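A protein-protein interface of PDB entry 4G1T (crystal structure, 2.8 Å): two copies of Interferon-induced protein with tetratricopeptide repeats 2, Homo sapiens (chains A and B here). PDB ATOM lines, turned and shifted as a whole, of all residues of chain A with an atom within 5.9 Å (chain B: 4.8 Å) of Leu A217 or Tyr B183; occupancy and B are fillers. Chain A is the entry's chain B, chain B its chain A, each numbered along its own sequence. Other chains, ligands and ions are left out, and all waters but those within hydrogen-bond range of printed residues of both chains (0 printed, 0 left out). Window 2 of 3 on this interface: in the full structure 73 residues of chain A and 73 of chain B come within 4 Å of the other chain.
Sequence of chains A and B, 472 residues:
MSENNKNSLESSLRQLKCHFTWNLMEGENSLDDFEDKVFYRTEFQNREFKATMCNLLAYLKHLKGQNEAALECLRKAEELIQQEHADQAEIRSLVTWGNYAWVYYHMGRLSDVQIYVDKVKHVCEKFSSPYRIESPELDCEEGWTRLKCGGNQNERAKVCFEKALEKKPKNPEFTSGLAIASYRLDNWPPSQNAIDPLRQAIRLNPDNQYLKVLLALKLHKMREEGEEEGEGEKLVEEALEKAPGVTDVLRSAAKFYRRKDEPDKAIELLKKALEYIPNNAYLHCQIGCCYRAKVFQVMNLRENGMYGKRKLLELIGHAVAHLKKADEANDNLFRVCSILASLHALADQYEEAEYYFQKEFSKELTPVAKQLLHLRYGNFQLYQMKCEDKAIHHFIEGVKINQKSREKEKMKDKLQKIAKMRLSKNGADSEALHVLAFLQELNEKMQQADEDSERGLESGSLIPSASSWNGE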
ATOM      1  N   ALA A 194      17.950 -20.109  -7.912  1.00  0.00           N
ATOM      2  CA  ALA A 194      18.385 -19.622  -6.608  1.00  0.00           C
ATOM      3  C   ALA A 194      17.201 -19.307  -5.677  1.00  0.00           C
ATOM      4  O   ALA A 194      17.364 -19.209  -4.447  1.00  0.00           O
ATOM      5  CB  ALA A 194      19.295 -18.400  -6.771  1.00  0.00           C
ATOM      6  N   LEU A 198      16.833 -20.471  -1.429  1.00  0.00           N
ATOM      7  CA  LEU A 198      16.741 -19.350  -0.512  1.00  0.00           C
ATOM      8  C   LEU A 198      15.548 -19.469   0.438  1.00  0.00           C
ATOM      9  O   LEU A 198      15.677 -19.295   1.657  1.00  0.00           O
ATOM     10  CB  LEU A 198      16.679 -18.037  -1.298  1.00  0.00           C
ATOM     11  CG  LEU A 198      18.002 -17.372  -1.702  1.00  0.00           C
ATOM     12  CD1 LEU A 198      17.791 -16.428  -2.871  1.00  0.00           C
ATOM     13  CD2 LEU A 198      18.602 -16.630  -0.528  1.00  0.00           C
ATOM     14  N   TYR A 210      20.122 -11.897   6.628  1.00  0.00           N
ATOM     15  CA  TYR A 210      20.784 -11.777   5.328  1.00  0.00           C
ATOM     16  C   TYR A 210      20.089 -12.566   4.213  1.00  0.00           C
ATOM     17  O   TYR A 210      19.880 -12.038   3.133  1.00  0.00           O
ATOM     18  CB  TYR A 210      22.272 -12.166   5.426  1.00  0.00           C
ATOM     19  CG  TYR A 210      23.067 -12.002   4.135  1.00  0.00           C
ATOM     20  CD1 TYR A 210      23.161 -10.777   3.503  1.00  0.00           C
ATOM     21  CD2 TYR A 210      23.736 -13.076   3.568  1.00  0.00           C
ATOM     22  CE1 TYR A 210      23.878 -10.633   2.341  1.00  0.00           C
ATOM     23  CE2 TYR A 210      24.451 -12.944   2.406  1.00  0.00           C
ATOM     24  CZ  TYR A 210      24.526 -11.719   1.796  1.00  0.00           C
ATOM     25  OH  TYR A 210      25.267 -11.584   0.630  1.00  0.00           O
ATOM     26  N   LYS A 212      17.046 -13.328   3.850  1.00  0.00           N
ATOM     27  CA  LYS A 212      15.790 -12.657   3.509  1.00  0.00           C
ATOM     28  C   LYS A 212      16.031 -11.519   2.522  1.00  0.00           C
ATOM     29  O   LYS A 212      15.332 -11.414   1.504  1.00  0.00           O
ATOM     30  CB  LYS A 212      15.054 -12.146   4.758  1.00  0.00           C
ATOM     31  CG  LYS A 212      14.443 -13.217   5.682  1.00  0.00           C
ATOM     32  CD  LYS A 212      13.774 -12.531   6.875  1.00  0.00           C
ATOM     33  CE  LYS A 212      13.231 -13.503   7.893  1.00  0.00           C
ATOM     34  NZ  LYS A 212      14.274 -13.978   8.824  1.00  0.00           N
ATOM     35  N   VAL A 213      17.019 -10.673   2.810  1.00  0.00           N
ATOM     36  CA  VAL A 213      17.377  -9.634   1.855  1.00  0.00           C
ATOM     37  C   VAL A 213      17.796 -10.210   0.510  1.00  0.00           C
ATOM     38  O   VAL A 213      17.455  -9.668  -0.525  1.00  0.00           O
ATOM     39  CB  VAL A 213      18.467  -8.695   2.377  1.00  0.00           C
ATOM     40  CG1 VAL A 213      18.703  -7.595   1.379  1.00  0.00           C
ATOM     41  CG2 VAL A 213      18.048  -8.091   3.722  1.00  0.00           C
ATOM     42  N   LEU A 214      18.507 -11.327   0.511  1.00  0.00           N
ATOM     43  CA  LEU A 214      18.919 -11.925  -0.753  1.00  0.00           C
ATOM     44  C   LEU A 214      17.710 -12.370  -1.538  1.00  0.00           C
ATOM     45  O   LEU A 214      17.628 -12.143  -2.739  1.00  0.00           O
ATOM     46  CB  LEU A 214      19.871 -13.106  -0.550  1.00  0.00           C
ATOM     47  CG  LEU A 214      21.302 -12.877  -0.063  1.00  0.00           C
ATOM     48  CD1 LEU A 214      22.096 -14.162  -0.170  1.00  0.00           C
ATOM     49  CD2 LEU A 214      21.983 -11.772  -0.849  1.00  0.00           C
ATOM     50  N   LEU A 215      16.771 -13.024  -0.867  1.00  0.00           N
ATOM     51  CA  LEU A 215      15.571 -13.484  -1.557  1.00  0.00           C
ATOM     52  C   LEU A 215      14.824 -12.291  -2.155  1.00  0.00           C
ATOM     53  O   LEU A 215      14.354 -12.345  -3.301  1.00  0.00           O
ATOM     54  CB  LEU A 215      14.681 -14.294  -0.616  1.00  0.00           C
ATOM     55  CG  LEU A 215      13.449 -15.037  -1.165  1.00  0.00           C
ATOM     56  CD1 LEU A 215      12.174 -14.358  -0.712  1.00  0.00           C
ATOM     57  CD2 LEU A 215      13.487 -15.175  -2.682  1.00  0.00           C
ATOM     58  N   ALA A 216      14.760 -11.203  -1.393  1.00  0.00           N
ATOM     59  CA  ALA A 216      14.064 -10.004  -1.837  1.00  0.00           C
ATOM     60  C   ALA A 216      14.663  -9.412  -3.118  1.00  0.00           C
ATOM     61  O   ALA A 216      13.933  -8.922  -3.978  1.00  0.00           O
ATOM     62  CB  ALA A 216      14.031  -8.972  -0.718  1.00  0.00           C
ATOM     63  N   LEU A 217      15.987  -9.466  -3.238  1.00  0.00           N
ATOM     64  CA  LEU A 217      16.689  -8.900  -4.381  1.00  0.00           C
ATOM     65  C   LEU A 217      16.532  -9.765  -5.586  1.00  0.00           C
ATOM     66  O   LEU A 217      16.722  -9.314  -6.706  1.00  0.00           O
ATOM     67  CB  LEU A 217      18.183  -8.820  -4.107  1.00  0.00           C
ATOM     68  CG  LEU A 217      18.710  -7.753  -3.158  1.00  0.00           C
ATOM     69  CD1 LEU A 217      19.997  -8.243  -2.534  1.00  0.00           C
ATOM     70  CD2 LEU A 217      18.877  -6.404  -3.868  1.00  0.00           C
ATOM     71  N   LYS A 218      16.229 -11.033  -5.362  1.00  0.00           N
ATOM     72  CA  LYS A 218      16.039 -11.933  -6.480  1.00  0.00           C
ATOM     73  C   LYS A 218      14.606 -11.832  -6.976  1.00  0.00           C
ATOM     74  O   LYS A 218      14.364 -11.899  -8.179  1.00  0.00           O
ATOM     75  CB  LYS A 218      16.410 -13.361  -6.096  1.00  0.00           C
ATOM     76  CG  LYS A 218      16.254 -14.373  -7.225  1.00  0.00           C
ATOM     77  CD  LYS A 218      16.963 -13.932  -8.500  1.00  0.00           C
ATOM     78  CE  LYS A 218      16.869 -15.000  -9.595  1.00  0.00           C
ATOM     79  NZ  LYS A 218      17.829 -16.134  -9.379  1.00  0.00           N
ATOM     80  N   LEU A 219      13.665 -11.645  -6.049  1.00  0.00           N
ATOM     81  CA  LEU A 219      12.247 -11.441  -6.404  1.00  0.00           C
ATOM     82  C   LEU A 219      12.049 -10.178  -7.226  1.00  0.00           C
ATOM     83  O   LEU A 219      11.589 -10.243  -8.362  1.00  0.00           O
ATOM     84  CB  LEU A 219      11.365 -11.353  -5.160  1.00  0.00           C
ATOM     85  CG  LEU A 219      11.241 -12.570  -4.240  1.00  0.00           C
ATOM     86  CD1 LEU A 219      10.667 -12.155  -2.887  1.00  0.00           C
ATOM     87  CD2 LEU A 219      10.422 -13.682  -4.892  1.00  0.00           C
ATOM     88  N   HIS A 220      12.384  -9.031  -6.637  1.00  0.00           N
ATOM     89  CA  HIS A 220      12.325  -7.749  -7.342  1.00  0.00           C
ATOM     90  C   HIS A 220      13.013  -7.777  -8.706  1.00  0.00           C
ATOM     91  O   HIS A 220      12.673  -6.999  -9.592  1.00  0.00           O
ATOM     92  CB  HIS A 220      12.946  -6.635  -6.503  1.00  0.00           C
ATOM     93  CG  HIS A 220      13.158  -5.360  -7.264  1.00  0.00           C
ATOM     94  ND1 HIS A 220      14.019  -5.271  -8.342  1.00  0.00           N
ATOM     95  CD2 HIS A 220      12.619  -4.129  -7.111  1.00  0.00           C
ATOM     96  CE1 HIS A 220      13.993  -4.040  -8.820  1.00  0.00           C
ATOM     97  NE2 HIS A 220      13.159  -3.326  -8.089  1.00  0.00           N
ATOM     98  N   LYS A 221      13.994  -8.655  -8.866  1.00  0.00           N
ATOM     99  CA  LYS A 221      14.727  -8.767 -10.120  1.00  0.00           C
ATOM    100  C   LYS A 221      13.965  -9.632 -11.119  1.00  0.00           C
ATOM    101  O   LYS A 221      14.365  -9.765 -12.275  1.00  0.00           O
ATOM    102  CB  LYS A 221      16.111  -9.358  -9.858  1.00  0.00           C
ATOM    103  CG  LYS A 221      17.031  -9.413 -11.062  1.00  0.00           C
ATOM    104  CD  LYS A 221      18.271 -10.231 -10.726  1.00  0.00           C
ATOM    105  CE  LYS A 221      19.288 -10.223 -11.848  1.00  0.00           C
ATOM    106  NZ  LYS A 221      20.333 -11.254 -11.616  1.00  0.00           N
ATOM    107  N   MET A 222      12.863 -10.214 -10.660  1.00  0.00           N
ATOM    108  CA  MET A 222      12.005 -11.032 -11.513  1.00  0.00           C
ATOM    109  C   MET A 222      10.621 -10.412 -11.729  1.00  0.00           C
ATOM    110  O   MET A 222       9.777 -11.011 -12.393  1.00  0.00           O
ATOM    111  CB  MET A 222      11.844 -12.439 -10.922  1.00  0.00           C
ATOM    112  CG  MET A 222      13.143 -13.054 -10.408  1.00  0.00           C
ATOM    113  SD  MET A 222      14.462 -13.071 -11.640  1.00  0.00           S
ATOM    114  CE  MET A 222      14.162 -14.638 -12.461  1.00  0.00           C
ATOM    115  N   SER A 252      23.095  -5.003   1.730  1.00  0.00           N
ATOM    116  CA  SER A 252      22.249  -5.578   0.682  1.00  0.00           C
ATOM    117  C   SER A 252      20.885  -4.945   0.630  1.00  0.00           C
ATOM    118  O   SER A 252      20.304  -4.830  -0.441  1.00  0.00           O
ATOM    119  CB  SER A 252      22.112  -7.092   0.801  1.00  0.00           C
ATOM    120  OG  SER A 252      22.103  -7.485   2.155  1.00  0.00           O
ATOM    121  N   ALA A 253      20.365  -4.526   1.775  1.00  0.00           N
ATOM    122  CA  ALA A 253      19.115  -3.775   1.775  1.00  0.00           C
ATOM    123  C   ALA A 253      19.280  -2.490   0.957  1.00  0.00           C
ATOM    124  O   ALA A 253      18.463  -2.191   0.091  1.00  0.00           O
ATOM    125  CB  ALA A 253      18.658  -3.472   3.200  1.00  0.00           C
ATOM    126  N   LYS A 255      21.255  -1.933  -1.510  1.00  0.00           N
ATOM    127  CA  LYS A 255      21.238  -2.310  -2.916  1.00  0.00           C
ATOM    128  C   LYS A 255      19.792  -2.490  -3.394  1.00  0.00           C
ATOM    129  O   LYS A 255      19.413  -2.058  -4.484  1.00  0.00           O
ATOM    130  CB  LYS A 255      22.043  -3.597  -3.108  1.00  0.00           C
ATOM    131  CG  LYS A 255      22.697  -3.781  -4.467  1.00  0.00           C
ATOM    132  CD  LYS A 255      23.491  -5.078  -4.461  1.00  0.00           C
ATOM    133  CE  LYS A 255      24.510  -5.130  -3.285  1.00  0.00           C
ATOM    134  NZ  LYS A 255      24.867  -6.526  -2.798  1.00  0.00           N
ATOM    135  N   PHE A 256      18.985  -3.137  -2.565  1.00  0.00           N
ATOM    136  CA  PHE A 256      17.573  -3.338  -2.861  1.00  0.00           C
ATOM    137  C   PHE A 256      16.933  -1.995  -3.148  1.00  0.00           C
ATOM    138  O   PHE A 256      16.424  -1.760  -4.231  1.00  0.00           O
ATOM    139  CB  PHE A 256      16.893  -4.016  -1.663  1.00  0.00           C
ATOM    140  CG  PHE A 256      15.427  -4.284  -1.849  1.00  0.00           C
ATOM    141  CD1 PHE A 256      14.490  -3.617  -1.076  1.00  0.00           C
ATOM    142  CD2 PHE A 256      14.985  -5.221  -2.767  1.00  0.00           C
ATOM    143  CE1 PHE A 256      13.146  -3.865  -1.232  1.00  0.00           C
ATOM    144  CE2 PHE A 256      13.639  -5.469  -2.918  1.00  0.00           C
ATOM    145  CZ  PHE A 256      12.721  -4.785  -2.152  1.00  0.00           C
ATOM    146  N   TYR A 257      16.999  -1.101  -2.176  1.00  0.00           N
ATOM    147  CA  TYR A 257      16.382   0.197  -2.314  1.00  0.00           C
ATOM    148  C   TYR A 257      16.901   1.020  -3.489  1.00  0.00           C
ATOM    149  O   TYR A 257      16.119   1.733  -4.104  1.00  0.00           O
ATOM    150  CB  TYR A 257      16.477   0.977  -1.009  1.00  0.00           C
ATOM    151  CG  TYR A 257      15.592   0.409   0.080  1.00  0.00           C
ATOM    152  CD1 TYR A 257      14.246   0.137  -0.155  1.00  0.00           C
ATOM    153  CD2 TYR A 257      16.103   0.118   1.334  1.00  0.00           C
ATOM    154  CE1 TYR A 257      13.438  -0.397   0.837  1.00  0.00           C
ATOM    155  CE2 TYR A 257      15.302  -0.428   2.329  1.00  0.00           C
ATOM    156  CZ  TYR A 257      13.970  -0.679   2.078  1.00  0.00           C
ATOM    157  OH  TYR A 257      13.175  -1.202   3.074  1.00  0.00           O
ATOM    158  N   ARG A 259      17.917  -0.363  -6.320  1.00  0.00           N
ATOM    159  CA  ARG A 259      17.284  -1.068  -7.428  1.00  0.00           C
ATOM    160  C   ARG A 259      15.829  -0.623  -7.462  1.00  0.00           C
ATOM    161  O   ARG A 259      15.248  -0.431  -8.530  1.00  0.00           O
ATOM    162  CB  ARG A 259      17.374  -2.580  -7.229  1.00  0.00           C
ATOM    163  CG  ARG A 259      18.795  -3.109  -7.129  1.00  0.00           C
ATOM    164  CD  ARG A 259      19.589  -2.805  -8.389  1.00  0.00           C
ATOM    165  NE  ARG A 259      20.959  -3.303  -8.305  1.00  0.00           N
ATOM    166  CZ  ARG A 259      21.336  -4.516  -8.695  1.00  0.00           C
ATOM    167  NH1 ARG A 259      20.446  -5.361  -9.197  1.00  0.00           N
ATOM    168  NH2 ARG A 259      22.604  -4.886  -8.583  1.00  0.00           N
ATOM    169  N   ALA B 179      22.335 -21.587  -0.941  1.00  0.00           N
ATOM    170  CA  ALA B 179      21.510 -20.432  -1.309  1.00  0.00           C
ATOM    171  C   ALA B 179      22.351 -19.196  -1.628  1.00  0.00           C
ATOM    172  O   ALA B 179      22.198 -18.598  -2.696  1.00  0.00           O
ATOM    173  CB  ALA B 179      20.509 -20.116  -0.204  1.00  0.00           C
ATOM    174  N   ILE B 180      23.229 -18.809  -0.701  1.00  0.00           N
ATOM    175  CA  ILE B 180      24.162 -17.721  -0.957  1.00  0.00           C
ATOM    176  C   ILE B 180      24.986 -17.996  -2.222  1.00  0.00           C
ATOM    177  O   ILE B 180      25.093 -17.141  -3.116  1.00  0.00           O
ATOM    178  CB  ILE B 180      25.095 -17.476   0.239  1.00  0.00           C
ATOM    179  CG1 ILE B 180      24.288 -17.016   1.451  1.00  0.00           C
ATOM    180  CG2 ILE B 180      26.142 -16.415  -0.112  1.00  0.00           C
ATOM    181  CD1 ILE B 180      25.065 -16.949   2.741  1.00  0.00           C
ATOM    182  N   ALA B 181      25.551 -19.193  -2.309  1.00  0.00           N
ATOM    183  CA  ALA B 181      26.328 -19.549  -3.479  1.00  0.00           C
ATOM    184  C   ALA B 181      25.534 -19.365  -4.763  1.00  0.00           C
ATOM    185  O   ALA B 181      26.014 -18.766  -5.724  1.00  0.00           O
ATOM    186  CB  ALA B 181      26.796 -20.963  -3.371  1.00  0.00           C
ATOM    187  N   SER B 182      24.311 -19.885  -4.766  1.00  0.00           N
ATOM    188  CA  SER B 182      23.467 -19.873  -5.951  1.00  0.00           C
ATOM    189  C   SER B 182      23.090 -18.452  -6.354  1.00  0.00           C
ATOM    190  O   SER B 182      23.173 -18.074  -7.531  1.00  0.00           O
ATOM    191  CB  SER B 182      22.213 -20.698  -5.687  1.00  0.00           C
ATOM    192  OG  SER B 182      22.570 -22.010  -5.293  1.00  0.00           O
ATOM    193  N   TYR B 183      22.674 -17.668  -5.363  1.00  0.00           N
ATOM    194  CA  TYR B 183      22.315 -16.273  -5.600  1.00  0.00           C
ATOM    195  C   TYR B 183      23.449 -15.541  -6.274  1.00  0.00           C
ATOM    196  O   TYR B 183      23.214 -14.754  -7.193  1.00  0.00           O
ATOM    197  CB  TYR B 183      21.964 -15.543  -4.299  1.00  0.00           C
ATOM    198  CG  TYR B 183      21.913 -14.040  -4.476  1.00  0.00           C
ATOM    199  CD1 TYR B 183      20.720 -13.401  -4.811  1.00  0.00           C
ATOM    200  CD2 TYR B 183      23.060 -13.259  -4.330  1.00  0.00           C
ATOM    201  CE1 TYR B 183      20.662 -12.037  -4.993  1.00  0.00           C
ATOM    202  CE2 TYR B 183      23.011 -11.890  -4.503  1.00  0.00           C
ATOM    203  CZ  TYR B 183      21.809 -11.281  -4.835  1.00  0.00           C
ATOM    204  OH  TYR B 183      21.749  -9.915  -5.016  1.00  0.00           O
ATOM    205  N   ARG B 184      24.671 -15.791  -5.789  1.00  0.00           N
ATOM    206  CA  ARG B 184      25.881 -15.155  -6.336  1.00  0.00           C
ATOM    207  C   ARG B 184      26.148 -15.663  -7.735  1.00  0.00           C
ATOM    208  O   ARG B 184      26.551 -14.902  -8.614  1.00  0.00           O
ATOM    209  CB  ARG B 184      27.099 -15.357  -5.417  1.00  0.00           C
ATOM    210  CG  ARG B 184      27.035 -14.509  -4.161  1.00  0.00           C
ATOM    211  CD  ARG B 184      28.244 -14.641  -3.300  1.00  0.00           C
ATOM    212  NE  ARG B 184      28.056 -13.953  -2.030  1.00  0.00           N
ATOM    213  CZ  ARG B 184      28.902 -14.038  -1.009  1.00  0.00           C
ATOM    214  NH1 ARG B 184      29.999 -14.780  -1.118  1.00  0.00           N
ATOM    215  NH2 ARG B 184      28.656 -13.386   0.125  1.00  0.00           N
ATOM    216  N   LEU B 185      25.869 -16.946  -7.938  1.00  0.00           N
ATOM    217  CA  LEU B 185      26.092 -17.576  -9.224  1.00  0.00           C
ATOM    218  C   LEU B 185      25.077 -17.129 -10.276  1.00  0.00           C
ATOM    219  O   LEU B 185      25.399 -17.059 -11.459  1.00  0.00           O
ATOM    220  CB  LEU B 185      26.093 -19.093  -9.081  1.00  0.00           C
ATOM    221  CG  LEU B 185      27.273 -19.760  -9.788  1.00  0.00           C
ATOM    222  CD1 LEU B 185      28.548 -19.532  -8.998  1.00  0.00           C
ATOM    223  CD2 LEU B 185      27.015 -21.237  -9.976  1.00  0.00           C
ATOM    224  N   ASP B 186      23.858 -16.810  -9.855  1.00  0.00           N
ATOM    225  CA  ASP B 186      22.899 -16.287 -10.813  1.00  0.00           C
ATOM    226  C   ASP B 186      23.130 -14.818 -11.117  1.00  0.00           C
ATOM    227  O   ASP B 186      22.965 -14.387 -12.255  1.00  0.00           O
ATOM    228  CB  ASP B 186      21.467 -16.472 -10.344  1.00  0.00           C
ATOM    229  CG  ASP B 186      20.479 -15.800 -11.275  1.00  0.00           C
ATOM    230  OD1 ASP B 186      20.436 -16.191 -12.468  1.00  0.00           O
ATOM    231  OD2 ASP B 186      19.768 -14.874 -10.820  1.00  0.00           O
ATOM    232  N   ASN B 187      23.493 -14.056 -10.089  1.00  0.00           N
ATOM    233  CA  ASN B 187      23.790 -12.625 -10.219  1.00  0.00           C
ATOM    234  C   ASN B 187      25.070 -12.319 -11.022  1.00  0.00           C
ATOM    235  O   ASN B 187      25.040 -11.553 -11.985  1.00  0.00           O
ATOM    236  CB  ASN B 187      23.885 -11.995  -8.829  1.00  0.00           C
ATOM    237  CG  ASN B 187      23.344 -10.585  -8.785  1.00  0.00           C
ATOM    238  OD1 ASN B 187      22.324 -10.281  -9.408  1.00  0.00           O
ATOM    239  ND2 ASN B 187      24.027  -9.708  -8.039  1.00  0.00           N
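Of the printed residues of chain B, Tyr A210 touches Arg B184 (3.9 Å). Of chain B, only Tyr B183 comes within 4 Å of Leu A217. Of the printed residues of chain B, Lys A221 touches Asp B186 (3.7 Å) and Asn B187 (3.1 Å). Ser A252 touches none of the printed residues of chain B. Phe A256 touches none of the printed residues of chain B. Printed residues of chain A within 4 Å of Ser B182: Ala A194. Tyr B183 touches just these residues of chain A: Ala A194 (3.7 Å), Leu A214 (3.8 Å) and Leu A217 (3.5 Å). Of the printed residues of chain A, Asp B186 touches Lys A218 (2.7 Å) and Lys A221 (3.7 Å). The nearest printed residue of chain A that does not touch Tyr B183 is Lys A218 (4.5 Å). The nearest printed residue of chain B that does not touch Tyr A210 is Ile B180 (4.1 Å).
Among the printed residues, merely in contact across the chains: Leu A217 with Tyr B183 (3.5 Å), Ala A194 with Tyr B183 (3.7 Å), Leu A214 with Tyr B183 (3.8 Å), Ala A194 with Ser B182 (3.8 Å), Leu A198 with Ala B179 (3.9 Å), Tyr A210 with Arg B184 (3.9 Å) and Leu A214 with Ile B180 (3.9 Å).
No position is printed for both chains.
The side-chain amino group of Lys A218 lies within salt-bridge range of the side-chain carboxylate of Asp B186, 2.7 Å away. The side-chain carboxylate (OD2) of Asp B186 lies within salt-bridge range of the side-chain amino group (NZ) of Lys A221, 3.7 Å away. The side-chain amide oxygen (OD1) of Asn B187 is in hydrogen-bond range of the side-chain amino group (NZ) of Lys A221 (3.1 Å).
Of the 20 printed residues of chain A, 7 touch a printed residue of chain B. Hydrophobic or aromatic side chains of chain A that line the printed part of chain B: Ala A194, Leu A198, Tyr A210, Leu A214 and Leu A217. Of the 9 printed residues of chain B, 7 touch a printed residue of chain A. Hydrophobic or aromatic side chains of chain B within 4 Å of the printed part of chain A: Ala B179, Ile B180 and Tyr B183. Along chain B the printed residues that touch a printed residue of chain A span positions 179 to 187. Among the printed residues, Asp or Glu carboxylates within 4 Å of a Lys or Arg side-chain nitrogen of the other chain: Lys A218 with Asp B186 (2.7 Å) and Lys A221 with Asp B186 (3.7 Å).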
